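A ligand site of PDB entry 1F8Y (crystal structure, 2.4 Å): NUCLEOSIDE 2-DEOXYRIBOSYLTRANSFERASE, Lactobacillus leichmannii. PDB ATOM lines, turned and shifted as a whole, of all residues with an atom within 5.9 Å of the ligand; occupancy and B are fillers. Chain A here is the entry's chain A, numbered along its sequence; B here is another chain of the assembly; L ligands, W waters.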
ATOM      1  N   TYR A   7      18.180  34.529  24.248  1.00  0.00           N
ATOM      2  CA  TYR A   7      18.658  33.151  24.174  1.00  0.00           C
ATOM      3  C   TYR A   7      18.355  32.856  22.698  1.00  0.00           C
ATOM      4  O   TYR A   7      17.199  33.000  22.275  1.00  0.00           O
ATOM      5  CB  TYR A   7      17.852  32.215  25.087  1.00  0.00           C
ATOM      6  CG  TYR A   7      18.127  30.745  24.821  1.00  0.00           C
ATOM      7  CD1 TYR A   7      19.049  30.027  25.585  1.00  0.00           C
ATOM      8  CD2 TYR A   7      17.467  30.067  23.775  1.00  0.00           C
ATOM      9  CE1 TYR A   7      19.314  28.685  25.315  1.00  0.00           C
ATOM     10  CE2 TYR A   7      17.722  28.739  23.504  1.00  0.00           C
ATOM     11  CZ  TYR A   7      18.636  28.044  24.274  1.00  0.00           C
ATOM     12  OH  TYR A   7      18.864  26.718  24.023  1.00  0.00           O
ATOM     13  N   PHE A   8      19.377  32.487  21.928  1.00  0.00           N
ATOM     14  CA  PHE A   8      19.218  32.217  20.506  1.00  0.00           C
ATOM     15  C   PHE A   8      18.708  30.816  20.192  1.00  0.00           C
ATOM     16  O   PHE A   8      19.492  29.936  19.834  1.00  0.00           O
ATOM     17  CB  PHE A   8      20.554  32.443  19.785  1.00  0.00           C
ATOM     18  CG  PHE A   8      20.417  32.573  18.299  1.00  0.00           C
ATOM     19  CD1 PHE A   8      19.746  33.658  17.745  1.00  0.00           C
ATOM     20  CD2 PHE A   8      20.916  31.600  17.452  1.00  0.00           C
ATOM     21  CE1 PHE A   8      19.560  33.754  16.370  1.00  0.00           C
ATOM     22  CE2 PHE A   8      20.739  31.688  16.069  1.00  0.00           C
ATOM     23  CZ  PHE A   8      20.061  32.776  15.530  1.00  0.00           C
ATOM     24  N   GLY A   9      17.399  30.619  20.289  1.00  0.00           N
ATOM     25  CA  GLY A   9      16.826  29.315  20.009  1.00  0.00           C
ATOM     26  C   GLY A   9      16.693  29.064  18.520  1.00  0.00           C
ATOM     27  O   GLY A   9      15.823  29.607  17.870  1.00  0.00           O
ATOM     28  N   ALA A  10      17.572  28.241  17.972  1.00  0.00           N
ATOM     29  CA  ALA A  10      17.534  27.967  16.548  1.00  0.00           C
ATOM     30  C   ALA A  10      18.240  26.662  16.232  1.00  0.00           C
ATOM     31  O   ALA A  10      19.329  26.408  16.738  1.00  0.00           O
ATOM     32  CB  ALA A  10      18.191  29.112  15.792  1.00  0.00           C
ATOM     33  N   GLY A  11      17.597  25.824  15.429  1.00  0.00           N
ATOM     34  CA  GLY A  11      18.196  24.562  15.040  1.00  0.00           C
ATOM     35  C   GLY A  11      19.238  24.805  13.974  1.00  0.00           C
ATOM     36  O   GLY A  11      19.266  25.872  13.345  1.00  0.00           O
ATOM     37  N   TRP A  12      20.072  23.807  13.720  1.00  0.00           N
ATOM     38  CA  TRP A  12      21.125  23.917  12.718  1.00  0.00           C
ATOM     39  C   TRP A  12      21.305  22.549  12.081  1.00  0.00           C
ATOM     40  O   TRP A  12      22.433  22.130  11.781  1.00  0.00           O
ATOM     41  CB  TRP A  12      22.412  24.383  13.400  1.00  0.00           C
ATOM     42  CG  TRP A  12      22.876  23.502  14.533  1.00  0.00           C
ATOM     43  CD1 TRP A  12      23.700  22.407  14.436  1.00  0.00           C
ATOM     44  CD2 TRP A  12      22.623  23.688  15.937  1.00  0.00           C
ATOM     45  NE1 TRP A  12      23.968  21.905  15.686  1.00  0.00           N
ATOM     46  CE2 TRP A  12      23.311  22.667  16.623  1.00  0.00           C
ATOM     47  CE3 TRP A  12      21.876  24.616  16.674  1.00  0.00           C
ATOM     48  CZ2 TRP A  12      23.298  22.549  18.021  1.00  0.00           C
ATOM     49  CZ3 TRP A  12      21.848  24.502  18.052  1.00  0.00           C
ATOM     50  CH2 TRP A  12      22.552  23.470  18.715  1.00  0.00           C
ATOM     51  N   PHE A  13      20.187  21.879  11.844  1.00  0.00           N
ATOM     52  CA  PHE A  13      20.187  20.519  11.324  1.00  0.00           C
ATOM     53  C   PHE A  13      19.765  20.331   9.862  1.00  0.00           C
ATOM     54  O   PHE A  13      19.745  19.207   9.380  1.00  0.00           O
ATOM     55  CB  PHE A  13      19.318  19.652  12.225  1.00  0.00           C
ATOM     56  CG  PHE A  13      19.509  19.944  13.695  1.00  0.00           C
ATOM     57  CD1 PHE A  13      18.456  20.455  14.462  1.00  0.00           C
ATOM     58  CD2 PHE A  13      20.742  19.731  14.303  1.00  0.00           C
ATOM     59  CE1 PHE A  13      18.633  20.743  15.819  1.00  0.00           C
ATOM     60  CE2 PHE A  13      20.939  20.018  15.656  1.00  0.00           C
ATOM     61  CZ  PHE A  13      19.874  20.527  16.412  1.00  0.00           C
ATOM     62  N   PRO A  42      23.611  28.899  21.889  1.00  0.00           N
ATOM     63  CA  PRO A  42      23.818  27.468  22.143  1.00  0.00           C
ATOM     64  C   PRO A  42      25.053  26.884  21.474  1.00  0.00           C
ATOM     65  O   PRO A  42      25.893  26.269  22.128  1.00  0.00           O
ATOM     66  CB  PRO A  42      22.538  26.839  21.603  1.00  0.00           C
ATOM     67  CG  PRO A  42      21.517  27.882  21.888  1.00  0.00           C
ATOM     68  CD  PRO A  42      22.225  29.140  21.431  1.00  0.00           C
ATOM     69  N   LEU A  43      25.178  27.105  20.169  1.00  0.00           N
ATOM     70  CA  LEU A  43      26.280  26.565  19.396  1.00  0.00           C
ATOM     71  C   LEU A  43      27.663  26.906  19.955  1.00  0.00           C
ATOM     72  O   LEU A  43      28.601  26.146  19.743  1.00  0.00           O
ATOM     73  CB  LEU A  43      26.150  27.005  17.924  1.00  0.00           C
ATOM     74  CG  LEU A  43      26.594  25.996  16.859  1.00  0.00           C
ATOM     75  CD1 LEU A  43      26.082  24.591  17.183  1.00  0.00           C
ATOM     76  CD2 LEU A  43      26.089  26.425  15.502  1.00  0.00           C
ATOM     77  N   GLN A  46      28.107  24.458  23.847  1.00  0.00           N
ATOM     78  CA  GLN A  46      27.959  23.013  24.059  1.00  0.00           C
ATOM     79  C   GLN A  46      29.055  22.660  25.055  1.00  0.00           C
ATOM     80  O   GLN A  46      30.122  23.289  25.046  1.00  0.00           O
ATOM     81  CB  GLN A  46      28.174  22.233  22.755  1.00  0.00           C
ATOM     82  CG  GLN A  46      27.283  22.674  21.606  1.00  0.00           C
ATOM     83  CD  GLN A  46      25.814  22.494  21.923  1.00  0.00           C
ATOM     84  OE1 GLN A  46      25.139  23.438  22.307  1.00  0.00           O
ATOM     85  NE2 GLN A  46      25.306  21.275  21.755  1.00  0.00           N
ATOM     86  N   VAL A  52      28.350  17.451  19.037  1.00  0.00           N
ATOM     87  CA  VAL A  52      28.265  16.008  18.812  1.00  0.00           C
ATOM     88  C   VAL A  52      28.248  15.627  17.343  1.00  0.00           C
ATOM     89  O   VAL A  52      28.544  14.483  17.011  1.00  0.00           O
ATOM     90  CB  VAL A  52      27.034  15.366  19.471  1.00  0.00           C
ATOM     91  CG1 VAL A  52      27.175  15.375  20.969  1.00  0.00           C
ATOM     92  CG2 VAL A  52      25.770  16.079  19.034  1.00  0.00           C
ATOM     93  N   TRP A  64      28.196  14.811  28.993  1.00  0.00           N
ATOM     94  CA  TRP A  64      28.143  15.840  27.963  1.00  0.00           C
ATOM     95  C   TRP A  64      26.702  16.296  27.824  1.00  0.00           C
ATOM     96  O   TRP A  64      26.410  17.486  27.774  1.00  0.00           O
ATOM     97  CB  TRP A  64      28.637  15.295  26.613  1.00  0.00           C
ATOM     98  CG  TRP A  64      28.546  16.316  25.497  1.00  0.00           C
ATOM     99  CD1 TRP A  64      29.494  17.222  25.137  1.00  0.00           C
ATOM    100  CD2 TRP A  64      27.409  16.579  24.656  1.00  0.00           C
ATOM    101  NE1 TRP A  64      29.019  18.049  24.154  1.00  0.00           N
ATOM    102  CE2 TRP A  64      27.737  17.679  23.842  1.00  0.00           C
ATOM    103  CE3 TRP A  64      26.134  16.004  24.545  1.00  0.00           C
ATOM    104  CZ2 TRP A  64      26.840  18.226  22.912  1.00  0.00           C
ATOM    105  CZ3 TRP A  64      25.238  16.538  23.616  1.00  0.00           C
ATOM    106  CH2 TRP A  64      25.599  17.634  22.819  1.00  0.00           C
ATOM    107  N   THR A  68      25.368  20.211  28.808  1.00  0.00           N
ATOM    108  CA  THR A  68      24.867  20.996  27.698  1.00  0.00           C
ATOM    109  C   THR A  68      23.400  21.334  27.892  1.00  0.00           C
ATOM    110  O   THR A  68      22.980  22.470  27.665  1.00  0.00           O
ATOM    111  CB  THR A  68      25.077  20.247  26.368  1.00  0.00           C
ATOM    112  OG1 THR A  68      26.481  19.992  26.210  1.00  0.00           O
ATOM    113  CG2 THR A  68      24.604  21.072  25.194  1.00  0.00           C
ATOM    114  N   ASP A  72      22.054  25.148  28.566  1.00  0.00           N
ATOM    115  CA  ASP A  72      20.995  25.731  27.742  1.00  0.00           C
ATOM    116  C   ASP A  72      19.902  26.307  28.654  1.00  0.00           C
ATOM    117  O   ASP A  72      19.472  27.473  28.475  1.00  0.00           O
ATOM    118  CB  ASP A  72      20.398  24.681  26.774  1.00  0.00           C
ATOM    119  CG  ASP A  72      21.303  24.361  25.574  1.00  0.00           C
ATOM    120  OD1 ASP A  72      22.384  24.969  25.383  1.00  0.00           O
ATOM    121  OD2 ASP A  72      20.908  23.474  24.786  1.00  0.00           O
ATOM    122  N   MET A  82      13.264  35.132  24.878  1.00  0.00           N
ATOM    123  CA  MET A  82      13.372  33.806  24.287  1.00  0.00           C
ATOM    124  C   MET A  82      13.102  33.974  22.793  1.00  0.00           C
ATOM    125  O   MET A  82      11.973  34.231  22.397  1.00  0.00           O
ATOM    126  CB  MET A  82      12.342  32.845  24.899  1.00  0.00           C
ATOM    127  CG  MET A  82      12.269  31.445  24.225  1.00  0.00           C
ATOM    128  SD  MET A  82      13.840  30.510  24.226  1.00  0.00           S
ATOM    129  CE  MET A  82      13.753  29.637  22.649  1.00  0.00           C
ATOM    130  N   ASP A  92      11.221  22.067  15.116  1.00  0.00           N
ATOM    131  CA  ASP A  92      12.170  21.415  16.010  1.00  0.00           C
ATOM    132  C   ASP A  92      11.672  21.070  17.398  1.00  0.00           C
ATOM    133  O   ASP A  92      11.334  21.958  18.190  1.00  0.00           O
ATOM    134  CB  ASP A  92      13.408  22.289  16.122  1.00  0.00           C
ATOM    135  CG  ASP A  92      14.540  21.587  16.818  1.00  0.00           C
ATOM    136  OD1 ASP A  92      14.927  22.055  17.890  1.00  0.00           O
ATOM    137  OD2 ASP A  92      15.034  20.560  16.295  1.00  0.00           O
ATOM    138  N   VAL A  93      11.704  19.779  17.737  1.00  0.00           N
ATOM    139  CA  VAL A  93      11.272  19.303  19.053  1.00  0.00           C
ATOM    140  C   VAL A  93      12.069  19.981  20.174  1.00  0.00           C
ATOM    141  O   VAL A  93      11.522  20.326  21.224  1.00  0.00           O
ATOM    142  CB  VAL A  93      11.361  17.756  19.182  1.00  0.00           C
ATOM    143  CG1 VAL A  93      12.825  17.293  19.185  1.00  0.00           C
ATOM    144  CG2 VAL A  93      10.631  17.293  20.440  1.00  0.00           C
ATOM    145  N   GLY A  94      13.346  20.251  19.911  1.00  0.00           N
ATOM    146  CA  GLY A  94      14.189  20.887  20.905  1.00  0.00           C
ATOM    147  C   GLY A  94      13.723  22.300  21.190  1.00  0.00           C
ATOM    148  O   GLY A  94      13.607  22.708  22.352  1.00  0.00           O
ATOM    149  N   LEU A  95      13.413  23.037  20.122  1.00  0.00           N
ATOM    150  CA  LEU A  95      12.942  24.414  20.231  1.00  0.00           C
ATOM    151  C   LEU A  95      11.608  24.424  20.949  1.00  0.00           C
ATOM    152  O   LEU A  95      11.323  25.322  21.751  1.00  0.00           O
ATOM    153  CB  LEU A  95      12.801  25.053  18.844  1.00  0.00           C
ATOM    154  CG  LEU A  95      12.235  26.479  18.782  1.00  0.00           C
ATOM    155  CD1 LEU A  95      12.914  27.390  19.808  1.00  0.00           C
ATOM    156  CD2 LEU A  95      12.384  27.042  17.371  1.00  0.00           C
ATOM    157  N   GLU A  98      12.012  24.066  24.663  1.00  0.00           N
ATOM    158  CA  GLU A  98      12.533  25.337  25.142  1.00  0.00           C
ATOM    159  C   GLU A  98      11.492  26.425  25.226  1.00  0.00           C
ATOM    160  O   GLU A  98      11.595  27.297  26.084  1.00  0.00           O
ATOM    161  CB  GLU A  98      13.736  25.763  24.305  1.00  0.00           C
ATOM    162  CG  GLU A  98      14.966  24.917  24.588  1.00  0.00           C
ATOM    163  CD  GLU A  98      16.037  25.046  23.520  1.00  0.00           C
ATOM    164  OE1 GLU A  98      17.149  24.512  23.754  1.00  0.00           O
ATOM    165  OE2 GLU A  98      15.769  25.658  22.465  1.00  0.00           O
ATOM    166  N   ASN B 123      16.697  14.061  20.507  1.00  0.00           N
ATOM    167  CA  ASN B 123      17.126  15.432  20.777  1.00  0.00           C
ATOM    168  C   ASN B 123      17.544  15.631  22.223  1.00  0.00           C
ATOM    169  O   ASN B 123      16.870  15.145  23.151  1.00  0.00           O
ATOM    170  CB  ASN B 123      16.001  16.409  20.406  1.00  0.00           C
ATOM    171  CG  ASN B 123      16.445  17.858  20.492  1.00  0.00           C
ATOM    172  OD1 ASN B 123      16.751  18.374  21.564  1.00  0.00           O
ATOM    173  ND2 ASN B 123      16.507  18.527  19.351  1.00  0.00           N
ATOM    174  N   LEU B 124      18.641  16.357  22.404  1.00  0.00           N
ATOM    175  CA  LEU B 124      19.207  16.666  23.713  1.00  0.00           C
ATOM    176  C   LEU B 124      18.163  17.131  24.721  1.00  0.00           C
ATOM    177  O   LEU B 124      18.129  16.631  25.842  1.00  0.00           O
ATOM    178  CB  LEU B 124      20.303  17.719  23.570  1.00  0.00           C
ATOM    179  CG  LEU B 124      21.343  18.058  24.646  1.00  0.00           C
ATOM    180  CD1 LEU B 124      21.121  19.429  25.180  1.00  0.00           C
ATOM    181  CD2 LEU B 124      21.413  17.029  25.760  1.00  0.00           C
ATOM    182  N   MET B 125      17.284  18.049  24.310  1.00  0.00           N
ATOM    183  CA  MET B 125      16.265  18.565  25.238  1.00  0.00           C
ATOM    184  C   MET B 125      15.222  17.542  25.644  1.00  0.00           C
ATOM    185  O   MET B 125      14.825  17.514  26.805  1.00  0.00           O
ATOM    186  CB  MET B 125      15.596  19.823  24.683  1.00  0.00           C
ATOM    187  CG  MET B 125      16.569  20.843  24.088  1.00  0.00           C
ATOM    188  SD  MET B 125      18.018  21.175  25.117  1.00  0.00           S
ATOM    189  CE  MET B 125      17.292  22.207  26.404  1.00  0.00           C
ATOM    190  N   TYR B 157      21.597  13.342  20.360  1.00  0.00           N
ATOM    191  CA  TYR B 157      22.292  14.307  19.501  1.00  0.00           C
ATOM    192  C   TYR B 157      22.071  15.727  19.983  1.00  0.00           C
ATOM    193  O   TYR B 157      22.784  16.619  19.470  1.00  0.00           O
ATOM    194  CB  TYR B 157      21.850  14.161  18.036  1.00  0.00           C
ATOM    195  CG  TYR B 157      20.440  14.644  17.748  1.00  0.00           C
ATOM    196  CD1 TYR B 157      20.199  15.985  17.436  1.00  0.00           C
ATOM    197  CD2 TYR B 157      19.354  13.767  17.780  1.00  0.00           C
ATOM    198  CE1 TYR B 157      18.916  16.446  17.169  1.00  0.00           C
ATOM    199  CE2 TYR B 157      18.069  14.220  17.508  1.00  0.00           C
ATOM    200  CZ  TYR B 157      17.864  15.565  17.217  1.00  0.00           C
ATOM    201  OH  TYR B 157      16.608  16.047  16.985  1.00  0.00           O
ATOM    202  OXT TYR B 157      21.165  15.947  20.835  1.00  0.00           O
HETATM  203  O1  LIG L   1      17.164  21.505  18.985  1.00  0.00           O
HETATM  204  C1  LIG L   1      17.910  22.753  18.814  1.00  0.00           C
HETATM  205  C2  LIG L   1      17.611  23.691  20.000  1.00  0.00           C
HETATM  206  O2  LIG L   1      17.804  22.971  21.192  1.00  0.00           O
HETATM  207  C3  LIG L   1      19.164  23.103  21.702  1.00  0.00           C
HETATM  208  C4  LIG L   1      20.140  21.957  21.400  1.00  0.00           C
HETATM  209  C5  LIG L   1      19.698  20.881  20.697  1.00  0.00           C
HETATM  210  C6  LIG L   1      21.551  22.038  21.813  1.00  0.00           C
HETATM  211  O3  LIG L   1      22.116  22.847  22.536  1.00  0.00           O
HETATM  212  N1  LIG L   1      22.294  20.957  21.416  1.00  0.00           N
HETATM  213  C7  LIG L   1      21.861  19.873  20.705  1.00  0.00           C
HETATM  214  O4  LIG L   1      22.697  19.108  20.295  1.00  0.00           O
HETATM  215  N2  LIG L   1      20.532  19.852  20.345  1.00  0.00           N
HETATM  216  C8  LIG L   1      19.964  18.721  19.626  1.00  0.00           C
HETATM  217  C9  LIG L   1      18.498  24.883  20.124  1.00  0.00           C
HETATM  218  O5  LIG L   1      17.811  25.923  20.795  1.00  0.00           O
HETATM  219  C10 LIG L   1      19.566  24.423  21.086  1.00  0.00           C
HETATM  220  O   HOH W   1      25.952  19.445  19.622  1.00  0.00           O
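Water W1 lies within hydrogen-bond range of NE2 of Gln 46 (2.9 Å), N of Val 52 (3.2 Å) and O4 of the ligand (3.3 Å).
The backbone NH (N) of Met 125 of chain B sits at hydrogen-bond distance from the side-chain amide oxygen (OD1) of Asn 123 of chain B (2.8 Å).
The side-chain carboxylate of Asp 92 lies within hydrogen-bond range of the backbone NH of Leu 95.
The side-chain amide nitrogen of Asn 123 of chain B is in hydrogen-bond range of the side-chain hydroxyl of Tyr 157 of chain B, at 3.4 Å.
OXT of Tyr 157 of chain B lies within hydrogen-bond range of N of Leu 124 of chain B, at 3.0 Å.
The side-chain carboxylate (OD1) of Asp 92 sits close to the backbone NH (N) of Gly 94 (3.1 Å).
The side-chain hydroxyl of Tyr 7 is in hydrogen-bond range of the side-chain carboxylate of Glu 98 (2.8 Å).
The backbone carbonyl oxygen of Pro 42 sits close to the side-chain amide oxygen of Gln 46 (2.9 Å).
The side-chain hydroxyl (OH) of Tyr 7 lies within hydrogen-bond range of an oxygen (O5) of the ligand.
ND2 of Asn 123 of chain B is in hydrogen-bond range of O1 of the ligand (3.1 Å).
OD1 of Asp 92 is in hydrogen-bond range of O1 of the ligand (2.6 Å).
A nitrogen (N1) of the ligand lies close to the side-chain amide nitrogen (NE2) of Gln 46, 3.0 Å away.
The side-chain carboxylate (OD2) of Asp 72 sits close to an oxygen (O3) of the ligand (2.6 Å).
An oxygen (O4) of the ligand sits close to the chain-end carboxylate (O) of Tyr 157 of chain B, 2.6 Å away.
The side-chain carboxylate (OE2) of Glu 98 sits at hydrogen-bond distance from an oxygen (O5) of the ligand, 2.7 Å away.
Residues that only touch the ligand: Trp 12, Phe 13, Gly 94, Gly 9, Ala 10, Met 125 of chain B, Pro 42 and Leu 124 of chain B.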
